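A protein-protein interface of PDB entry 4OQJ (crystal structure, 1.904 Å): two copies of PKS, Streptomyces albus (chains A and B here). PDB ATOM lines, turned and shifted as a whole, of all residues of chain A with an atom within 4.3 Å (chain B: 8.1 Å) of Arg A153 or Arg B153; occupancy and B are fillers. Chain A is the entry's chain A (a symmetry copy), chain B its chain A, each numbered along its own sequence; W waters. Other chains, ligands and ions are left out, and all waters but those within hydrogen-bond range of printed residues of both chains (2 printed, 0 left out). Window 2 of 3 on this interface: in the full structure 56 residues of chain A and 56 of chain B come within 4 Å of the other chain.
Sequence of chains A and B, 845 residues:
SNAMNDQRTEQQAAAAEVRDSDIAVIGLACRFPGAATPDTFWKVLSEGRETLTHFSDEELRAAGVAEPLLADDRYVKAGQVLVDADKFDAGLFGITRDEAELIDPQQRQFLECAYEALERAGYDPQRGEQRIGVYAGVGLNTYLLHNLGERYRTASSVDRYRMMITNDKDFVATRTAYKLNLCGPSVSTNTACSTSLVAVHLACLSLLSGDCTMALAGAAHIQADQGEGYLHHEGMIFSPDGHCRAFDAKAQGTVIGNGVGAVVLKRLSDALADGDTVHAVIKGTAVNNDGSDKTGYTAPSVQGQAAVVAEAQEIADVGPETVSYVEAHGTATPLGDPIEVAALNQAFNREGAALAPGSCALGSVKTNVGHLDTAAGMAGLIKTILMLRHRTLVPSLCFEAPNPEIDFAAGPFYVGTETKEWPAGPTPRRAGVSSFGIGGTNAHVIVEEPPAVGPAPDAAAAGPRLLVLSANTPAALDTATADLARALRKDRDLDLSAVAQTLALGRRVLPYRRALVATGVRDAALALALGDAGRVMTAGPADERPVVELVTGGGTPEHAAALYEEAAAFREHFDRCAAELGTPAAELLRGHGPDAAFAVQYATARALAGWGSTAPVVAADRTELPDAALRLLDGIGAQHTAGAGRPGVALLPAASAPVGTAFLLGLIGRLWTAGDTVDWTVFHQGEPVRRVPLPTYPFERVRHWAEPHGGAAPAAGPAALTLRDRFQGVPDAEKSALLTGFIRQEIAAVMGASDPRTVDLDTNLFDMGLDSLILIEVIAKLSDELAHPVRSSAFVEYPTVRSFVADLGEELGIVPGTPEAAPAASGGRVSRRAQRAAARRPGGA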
ATOM      1  N   LEU A 145      14.290 -14.093   1.034  1.00  0.00           N
ATOM      2  CA  LEU A 145      15.602 -14.017   1.661  1.00  0.00           C
ATOM      3  C   LEU A 145      16.388 -15.326   1.535  1.00  0.00           C
ATOM      4  O   LEU A 145      17.584 -15.297   1.271  1.00  0.00           O
ATOM      5  CB  LEU A 145      15.451 -13.633   3.139  1.00  0.00           C
ATOM      6  CG  LEU A 145      14.924 -12.222   3.409  1.00  0.00           C
ATOM      7  CD1 LEU A 145      14.623 -12.003   4.905  1.00  0.00           C
ATOM      8  CD2 LEU A 145      15.928 -11.205   2.909  1.00  0.00           C
ATOM      9  N   GLY A 149      17.207 -15.648  -2.411  1.00  0.00           N
ATOM     10  CA  GLY A 149      18.265 -14.738  -2.015  1.00  0.00           C
ATOM     11  C   GLY A 149      19.371 -14.616  -3.047  1.00  0.00           C
ATOM     12  O   GLY A 149      19.559 -13.552  -3.634  1.00  0.00           O
ATOM     13  N   GLU A 150      20.108 -15.700  -3.261  1.00  0.00           N
ATOM     14  CA  GLU A 150      21.238 -15.685  -4.186  1.00  0.00           C
ATOM     15  C   GLU A 150      20.755 -15.320  -5.582  1.00  0.00           C
ATOM     16  O   GLU A 150      21.407 -14.565  -6.303  1.00  0.00           O
ATOM     17  CB  GLU A 150      21.943 -17.045  -4.198  1.00  0.00           C
ATOM     18  N   ARG A 151      19.597 -15.862  -5.944  1.00  0.00           N
ATOM     19  CA  ARG A 151      18.971 -15.594  -7.229  1.00  0.00           C
ATOM     20  C   ARG A 151      18.825 -14.092  -7.458  1.00  0.00           C
ATOM     21  O   ARG A 151      19.137 -13.584  -8.530  1.00  0.00           O
ATOM     22  CB  ARG A 151      17.609 -16.281  -7.278  1.00  0.00           C
ATOM     23  CG  ARG A 151      17.064 -16.577  -8.656  1.00  0.00           C
ATOM     24  CD  ARG A 151      16.154 -17.798  -8.580  1.00  0.00           C
ATOM     25  NE  ARG A 151      15.057 -17.756  -9.538  1.00  0.00           N
ATOM     26  CZ  ARG A 151      14.108 -18.684  -9.624  1.00  0.00           C
ATOM     27  NH1 ARG A 151      14.123 -19.733  -8.810  1.00  0.00           N
ATOM     28  NH2 ARG A 151      13.144 -18.565 -10.528  1.00  0.00           N
ATOM     29  N   TYR A 152      18.345 -13.389  -6.430  1.00  0.00           N
ATOM     30  CA  TYR A 152      18.131 -11.943  -6.515  1.00  0.00           C
ATOM     31  C   TYR A 152      19.426 -11.150  -6.757  1.00  0.00           C
ATOM     32  O   TYR A 152      19.488 -10.322  -7.665  1.00  0.00           O
ATOM     33  CB  TYR A 152      17.459 -11.412  -5.240  1.00  0.00           C
ATOM     34  CG  TYR A 152      17.066  -9.951  -5.360  1.00  0.00           C
ATOM     35  CD1 TYR A 152      17.957  -8.932  -5.034  1.00  0.00           C
ATOM     36  CD2 TYR A 152      15.809  -9.592  -5.824  1.00  0.00           C
ATOM     37  CE1 TYR A 152      17.598  -7.596  -5.167  1.00  0.00           C
ATOM     38  CE2 TYR A 152      15.445  -8.267  -5.958  1.00  0.00           C
ATOM     39  CZ  TYR A 152      16.343  -7.275  -5.627  1.00  0.00           C
ATOM     40  OH  TYR A 152      15.971  -5.960  -5.767  1.00  0.00           O
ATOM     41  N   ARG A 153      20.450 -11.386  -5.945  1.00  0.00           N
ATOM     42  CA  ARG A 153      21.644 -10.543  -5.995  1.00  0.00           C
ATOM     43  C   ARG A 153      22.487 -10.753  -7.257  1.00  0.00           C
ATOM     44  O   ARG A 153      23.305  -9.902  -7.597  1.00  0.00           O
ATOM     45  CB  ARG A 153      22.509 -10.770  -4.754  1.00  0.00           C
ATOM     46  CG  ARG A 153      22.344  -9.678  -3.692  1.00  0.00           C
ATOM     47  CD  ARG A 153      22.715 -10.171  -2.304  1.00  0.00           C
ATOM     48  NE  ARG A 153      21.824 -11.257  -1.911  1.00  0.00           N
ATOM     49  CZ  ARG A 153      22.206 -12.494  -1.600  1.00  0.00           C
ATOM     50  NH1 ARG A 153      23.488 -12.844  -1.584  1.00  0.00           N
ATOM     51  NH2 ARG A 153      21.283 -13.387  -1.280  1.00  0.00           N
ATOM     52  N   THR A 154      22.270 -11.861  -7.957  1.00  0.00           N
ATOM     53  CA  THR A 154      23.003 -12.148  -9.192  1.00  0.00           C
ATOM     54  C   THR A 154      22.117 -12.057 -10.436  1.00  0.00           C
ATOM     55  O   THR A 154      22.457 -12.603 -11.483  1.00  0.00           O
ATOM     56  CB  THR A 154      23.628 -13.551  -9.155  1.00  0.00           C
ATOM     57  OG1 THR A 154      22.603 -14.532  -9.352  1.00  0.00           O
ATOM     58  CG2 THR A 154      24.338 -13.796  -7.822  1.00  0.00           C
ATOM     59  N   ALA A 155      20.983 -11.371 -10.315  1.00  0.00           N
ATOM     60  CA  ALA A 155      20.030 -11.255 -11.416  1.00  0.00           C
ATOM     61  C   ALA A 155      20.031  -9.856 -12.024  1.00  0.00           C
ATOM     62  O   ALA A 155      20.480  -8.893 -11.400  1.00  0.00           O
ATOM     63  CB  ALA A 155      18.630 -11.609 -10.942  1.00  0.00           C
ATOM     64  N   ARG A 160      15.009  -8.984 -11.222  1.00  0.00           N
ATOM     65  CA  ARG A 160      14.802  -8.422  -9.893  1.00  0.00           C
ATOM     66  C   ARG A 160      13.418  -7.781  -9.782  1.00  0.00           C
ATOM     67  O   ARG A 160      12.717  -7.950  -8.785  1.00  0.00           O
ATOM     68  CB  ARG A 160      15.891  -7.401  -9.576  1.00  0.00           C
ATOM     69  CG  ARG A 160      17.224  -8.044  -9.219  1.00  0.00           C
ATOM     70  CD  ARG A 160      18.275  -7.007  -8.919  1.00  0.00           C
ATOM     71  NE  ARG A 160      19.518  -7.625  -8.474  1.00  0.00           N
ATOM     72  CZ  ARG A 160      20.535  -6.954  -7.946  1.00  0.00           C
ATOM     73  NH1 ARG A 160      20.462  -5.637  -7.794  1.00  0.00           N
ATOM     74  NH2 ARG A 160      21.627  -7.600  -7.569  1.00  0.00           N
ATOM     75  N   THR B 142      15.871  -2.930  -0.194  1.00  0.00           N
ATOM     76  CA  THR B 142      17.064  -3.428  -0.862  1.00  0.00           C
ATOM     77  C   THR B 142      18.274  -3.365   0.080  1.00  0.00           C
ATOM     78  O   THR B 142      19.295  -3.982  -0.189  1.00  0.00           O
ATOM     79  CB  THR B 142      17.356  -2.641  -2.164  1.00  0.00           C
ATOM     80  OG1 THR B 142      17.265  -1.229  -1.919  1.00  0.00           O
ATOM     81  CG2 THR B 142      16.336  -3.029  -3.267  1.00  0.00           C
ATOM     82  N   LEU B 144      18.242  -4.580   3.164  1.00  0.00           N
ATOM     83  CA  LEU B 144      18.220  -5.910   3.736  1.00  0.00           C
ATOM     84  C   LEU B 144      18.724  -6.938   2.728  1.00  0.00           C
ATOM     85  O   LEU B 144      19.534  -7.801   3.052  1.00  0.00           O
ATOM     86  CB  LEU B 144      16.799  -6.256   4.193  1.00  0.00           C
ATOM     87  CG  LEU B 144      16.534  -7.687   4.653  1.00  0.00           C
ATOM     88  CD1 LEU B 144      17.313  -8.010   5.909  1.00  0.00           C
ATOM     89  CD2 LEU B 144      15.044  -7.886   4.874  1.00  0.00           C
ATOM     90  N   LEU B 145      18.246  -6.838   1.497  1.00  0.00           N
ATOM     91  CA  LEU B 145      18.609  -7.801   0.467  1.00  0.00           C
ATOM     92  C   LEU B 145      20.077  -7.687   0.050  1.00  0.00           C
ATOM     93  O   LEU B 145      20.741  -8.701  -0.134  1.00  0.00           O
ATOM     94  CB  LEU B 145      17.698  -7.623  -0.756  1.00  0.00           C
ATOM     95  CG  LEU B 145      16.224  -7.974  -0.543  1.00  0.00           C
ATOM     96  CD1 LEU B 145      15.363  -7.578  -1.760  1.00  0.00           C
ATOM     97  CD2 LEU B 145      16.094  -9.454  -0.255  1.00  0.00           C
ATOM     98  N   HIS B 146      20.578  -6.463  -0.116  1.00  0.00           N
ATOM     99  CA  HIS B 146      21.964  -6.251  -0.561  1.00  0.00           C
ATOM    100  C   HIS B 146      22.937  -6.168   0.614  1.00  0.00           C
ATOM    101  O   HIS B 146      23.752  -7.061   0.817  1.00  0.00           O
ATOM    102  CB  HIS B 146      22.095  -4.973  -1.389  1.00  0.00           C
ATOM    103  CG  HIS B 146      21.265  -4.953  -2.639  1.00  0.00           C
ATOM    104  ND1 HIS B 146      21.334  -3.923  -3.553  1.00  0.00           N
ATOM    105  CD2 HIS B 146      20.349  -5.825  -3.125  1.00  0.00           C
ATOM    106  CE1 HIS B 146      20.499  -4.160  -4.548  1.00  0.00           C
ATOM    107  NE2 HIS B 146      19.890  -5.307  -4.314  1.00  0.00           N
ATOM    108  N   ASN B 147      22.839  -5.090   1.388  1.00  0.00           N
ATOM    109  CA  ASN B 147      23.808  -4.805   2.445  1.00  0.00           C
ATOM    110  C   ASN B 147      23.822  -5.821   3.586  1.00  0.00           C
ATOM    111  O   ASN B 147      24.877  -6.111   4.146  1.00  0.00           O
ATOM    112  CB  ASN B 147      23.545  -3.414   3.019  1.00  0.00           C
ATOM    113  CG  ASN B 147      23.708  -2.326   1.984  1.00  0.00           C
ATOM    114  OD1 ASN B 147      22.905  -2.213   1.061  1.00  0.00           O
ATOM    115  ND2 ASN B 147      24.747  -1.513   2.136  1.00  0.00           N
ATOM    116  N   LEU B 148      22.653  -6.354   3.929  1.00  0.00           N
ATOM    117  CA  LEU B 148      22.516  -7.273   5.056  1.00  0.00           C
ATOM    118  C   LEU B 148      22.212  -8.698   4.610  1.00  0.00           C
ATOM    119  O   LEU B 148      22.027  -9.592   5.447  1.00  0.00           O
ATOM    120  CB  LEU B 148      21.404  -6.798   5.997  1.00  0.00           C
ATOM    121  CG  LEU B 148      21.560  -5.409   6.596  1.00  0.00           C
ATOM    122  CD1 LEU B 148      20.381  -5.117   7.513  1.00  0.00           C
ATOM    123  CD2 LEU B 148      22.865  -5.307   7.358  1.00  0.00           C
ATOM    124  N   GLY B 149      22.157  -8.900   3.298  1.00  0.00           N
ATOM    125  CA  GLY B 149      21.816 -10.191   2.729  1.00  0.00           C
ATOM    126  C   GLY B 149      22.638 -11.334   3.297  1.00  0.00           C
ATOM    127  O   GLY B 149      22.099 -12.213   3.969  1.00  0.00           O
ATOM    128  N   GLU B 150      23.937 -11.329   3.020  1.00  0.00           N
ATOM    129  CA  GLU B 150      24.816 -12.408   3.462  1.00  0.00           C
ATOM    130  C   GLU B 150      24.791 -12.504   4.980  1.00  0.00           C
ATOM    131  O   GLU B 150      24.774 -13.596   5.548  1.00  0.00           O
ATOM    132  CB  GLU B 150      26.245 -12.179   2.960  1.00  0.00           C
ATOM    133  N   ARG B 151      24.778 -11.342   5.624  1.00  0.00           N
ATOM    134  CA  ARG B 151      24.718 -11.246   7.074  1.00  0.00           C
ATOM    135  C   ARG B 151      23.540 -12.047   7.622  1.00  0.00           C
ATOM    136  O   ARG B 151      23.677 -12.793   8.586  1.00  0.00           O
ATOM    137  CB  ARG B 151      24.607  -9.779   7.478  1.00  0.00           C
ATOM    138  CG  ARG B 151      25.069  -9.439   8.876  1.00  0.00           C
ATOM    139  CD  ARG B 151      25.557  -7.995   8.902  1.00  0.00           C
ATOM    140  NE  ARG B 151      25.327  -7.333  10.179  1.00  0.00           N
ATOM    141  CZ  ARG B 151      25.624  -6.060  10.422  1.00  0.00           C
ATOM    142  NH1 ARG B 151      26.169  -5.308   9.473  1.00  0.00           N
ATOM    143  NH2 ARG B 151      25.379  -5.538  11.617  1.00  0.00           N
ATOM    144  N   TYR B 152      22.376 -11.879   6.990  1.00  0.00           N
ATOM    145  CA  TYR B 152      21.157 -12.566   7.420  1.00  0.00           C
ATOM    146  C   TYR B 152      21.256 -14.097   7.327  1.00  0.00           C
ATOM    147  O   TYR B 152      20.958 -14.800   8.291  1.00  0.00           O
ATOM    148  CB  TYR B 152      19.946 -12.099   6.599  1.00  0.00           C
ATOM    149  CG  TYR B 152      18.638 -12.659   7.128  1.00  0.00           C
ATOM    150  CD1 TYR B 152      18.155 -13.894   6.704  1.00  0.00           C
ATOM    151  CD2 TYR B 152      17.900 -11.961   8.072  1.00  0.00           C
ATOM    152  CE1 TYR B 152      16.968 -14.410   7.210  1.00  0.00           C
ATOM    153  CE2 TYR B 152      16.719 -12.468   8.578  1.00  0.00           C
ATOM    154  CZ  TYR B 152      16.259 -13.691   8.142  1.00  0.00           C
ATOM    155  OH  TYR B 152      15.085 -14.187   8.655  1.00  0.00           O
ATOM    156  N   ARG B 153      21.656 -14.616   6.171  1.00  0.00           N
ATOM    157  CA  ARG B 153      21.597 -16.060   5.948  1.00  0.00           C
ATOM    158  C   ARG B 153      22.633 -16.846   6.758  1.00  0.00           C
ATOM    159  O   ARG B 153      22.486 -18.052   6.936  1.00  0.00           O
ATOM    160  CB  ARG B 153      21.757 -16.376   4.460  1.00  0.00           C
ATOM    161  CG  ARG B 153      20.429 -16.677   3.758  1.00  0.00           C
ATOM    162  CD  ARG B 153      20.503 -16.420   2.263  1.00  0.00           C
ATOM    163  NE  ARG B 153      20.782 -15.010   2.017  1.00  0.00           N
ATOM    164  CZ  ARG B 153      21.837 -14.534   1.360  1.00  0.00           C
ATOM    165  NH1 ARG B 153      22.742 -15.343   0.817  1.00  0.00           N
ATOM    166  NH2 ARG B 153      21.974 -13.224   1.230  1.00  0.00           N
ATOM    167  N   THR B 154      23.655 -16.164   7.263  1.00  0.00           N
ATOM    168  CA  THR B 154      24.689 -16.814   8.074  1.00  0.00           C
ATOM    169  C   THR B 154      24.626 -16.402   9.546  1.00  0.00           C
ATOM    170  O   THR B 154      25.603 -16.554  10.276  1.00  0.00           O
ATOM    171  CB  THR B 154      26.095 -16.487   7.548  1.00  0.00           C
ATOM    172  OG1 THR B 154      26.436 -15.143   7.909  1.00  0.00           O
ATOM    173  CG2 THR B 154      26.160 -16.652   6.027  1.00  0.00           C
ATOM    174  N   ALA B 155      23.480 -15.880   9.974  1.00  0.00           N
ATOM    175  CA  ALA B 155      23.313 -15.402  11.345  1.00  0.00           C
ATOM    176  C   ALA B 155      22.425 -16.331  12.166  1.00  0.00           C
ATOM    177  O   ALA B 155      21.660 -17.127  11.618  1.00  0.00           O
ATOM    178  CB  ALA B 155      22.732 -13.998  11.347  1.00  0.00           C
ATOM    179  N   SER B 156      22.542 -16.213  13.485  1.00  0.00           N
ATOM    180  CA  SER B 156      21.693 -16.935  14.423  1.00  0.00           C
ATOM    181  C   SER B 156      20.247 -16.462  14.341  1.00  0.00           C
ATOM    182  O   SER B 156      19.941 -15.492  13.648  1.00  0.00           O
ATOM    183  CB  SER B 156      22.204 -16.743  15.847  1.00  0.00           C
ATOM    184  OG  SER B 156      22.220 -15.363  16.178  1.00  0.00           O
ATOM    185  N   ARG B 160      18.966 -12.709  13.407  1.00  0.00           N
ATOM    186  CA  ARG B 160      17.940 -12.618  12.375  1.00  0.00           C
ATOM    187  C   ARG B 160      16.710 -11.874  12.893  1.00  0.00           C
ATOM    188  O   ARG B 160      16.139 -11.031  12.202  1.00  0.00           O
ATOM    189  CB  ARG B 160      17.556 -14.012  11.888  1.00  0.00           C
ATOM    190  CG  ARG B 160      18.595 -14.627  10.959  1.00  0.00           C
ATOM    191  CD  ARG B 160      18.186 -16.004  10.505  1.00  0.00           C
ATOM    192  NE  ARG B 160      19.129 -16.544   9.533  1.00  0.00           N
ATOM    193  CZ  ARG B 160      18.910 -17.637   8.814  1.00  0.00           C
ATOM    194  NH1 ARG B 160      17.777 -18.315   8.951  1.00  0.00           N
ATOM    195  NH2 ARG B 160      19.825 -18.055   7.953  1.00  0.00           N
ATOM    196  N   MET B 163      17.414  -8.276  13.000  1.00  0.00           N
ATOM    197  CA  MET B 163      17.337  -7.731  11.651  1.00  0.00           C
ATOM    198  C   MET B 163      15.882  -7.606  11.163  1.00  0.00           C
ATOM    199  O   MET B 163      15.545  -6.653  10.480  1.00  0.00           O
ATOM    200  CB  MET B 163      18.163  -8.595  10.686  1.00  0.00           C
ATOM    201  CG  MET B 163      19.654  -8.244  10.742  1.00  0.00           C
ATOM    202  SD  MET B 163      20.727  -9.239   9.471  1.00  0.00           S
ATOM    203  CE  MET B 163      21.000 -10.797  10.588  1.00  0.00           C
ATOM    204  N   PRO B 708      28.180  -4.491   2.675  1.00  0.00           N
ATOM    205  CA  PRO B 708      27.840  -5.851   2.238  1.00  0.00           C
ATOM    206  C   PRO B 708      29.044  -6.785   2.229  1.00  0.00           C
ATOM    207  O   PRO B 708      29.196  -7.544   3.186  1.00  0.00           O
ATOM    208  CB  PRO B 708      27.296  -5.644   0.817  1.00  0.00           C
ATOM    209  CG  PRO B 708      27.842  -4.331   0.374  1.00  0.00           C
ATOM    210  CD  PRO B 708      27.977  -3.496   1.605  1.00  0.00           C
HETATM  211  O   HOH W   1      19.475 -11.407  -0.628  1.00  0.00           O
HETATM  212  O   HOH W   2      19.278 -12.819   1.662  1.00  0.00           O
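The guanidinium group of Arg A153 lies close to the backbone carbonyl oxygen of Leu B145.
The guanidinium group (NE) of Arg B153 lies close to the backbone carbonyl oxygen (O) of Leu A145, at 3.3 Å.
NH2 of Arg B153 sits close to NH2 of Arg A153 (2.6 Å).
The backbone carbonyl oxygen (O) of Gly A149 lies close to the guanidinium group (NH2) of Arg A153, 2.9 Å away.
The backbone carbonyl oxygen of Ala A155 is in hydrogen-bond range of the guanidinium group of Arg A160, 3.3 Å away.
The guanidinium group of Arg B153 sits close to the backbone carbonyl oxygen of Gly B149.
The guanidinium group of Arg A160 is in hydrogen-bond range of the backbone carbonyl oxygen of Tyr A152 (2.8 Å).
The backbone carbonyl oxygen of Leu B144 is in hydrogen-bond range of the backbone NH of Gly B149, 2.9 Å away.
The guanidinium group of Arg B160 lies within hydrogen-bond range of the backbone carbonyl oxygen of Arg B153.
Among the printed residues, merely in contact across the chains: Tyr A152 with His B146 (3.3 Å), Arg A160 with His B146 (3.5 Å), Leu A145 with Leu B145 (3.6 Å), Tyr A152 with Thr B142 (3.9 Å) and Leu A145 with Leu B144 (3.96 Å).
Of the printed residues of chain A, Arg B153 touches Leu A145 and Arg A153.
Of the printed residues of chain A, Leu B144 touches Leu A145 (3.96 Å).
Printed residues of chain A within 4 Å of Thr B142: Tyr A152.
Printed residues of chain B within 4 Å of Leu A145: Leu B144, Leu B145 and Arg B153.
Printed residues of chain B within 4 Å of Tyr A152: Thr B142 (3.9 Å) and His B146 (3.3 Å).
Asn B147 touches none of the printed residues of chain A.
Arg B160 touches none of the printed residues of chain A.
The nearest printed residue of chain A that does not touch Leu B144 is Arg A153 (6.5 Å).
Of the 17 printed residues of chain B, 5 touch a printed residue of chain A.
Hydrophobic or aromatic side chains of chain B within 4 Å of the printed part of chain A: Leu B144, Leu B145 and His B146.
Of the 9 printed residues of chain A, 4 touch a printed residue of chain B.
Hydrophobic or aromatic side chains of chain A that line the printed part of chain B: Leu A145 and Tyr A152.
Among the printed residues, 8 pairs touch across the chains.
Among the printed residues, no Asp or Glu carboxylate lies within 4 Å of a Lys or Arg side-chain nitrogen of the other chain.
Leu A145 touches its own counterpart, Leu B145.
Leu A145 touches Arg B153, and with the chains exchanged Arg A153 touches Leu B145.
Arg B153 touches its own counterpart, Arg A153.
Positions printed for both chains: 145, 149, 150, 151, 152, 153, 154, 155 and 160.
Of the 8 pairs that touch across the chains among the printed residues, 4 have their exchanged pair printed and touching as well.
Water W2 bridges NE of Arg B153 (2.7 Å) and O of Leu A145 (3.0 Å).
Water W1 lies within hydrogen-bond range of the guanidinium group of Arg A153 (2.7 Å) and the backbone carbonyl oxygen of Leu B145 (3.0 Å).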
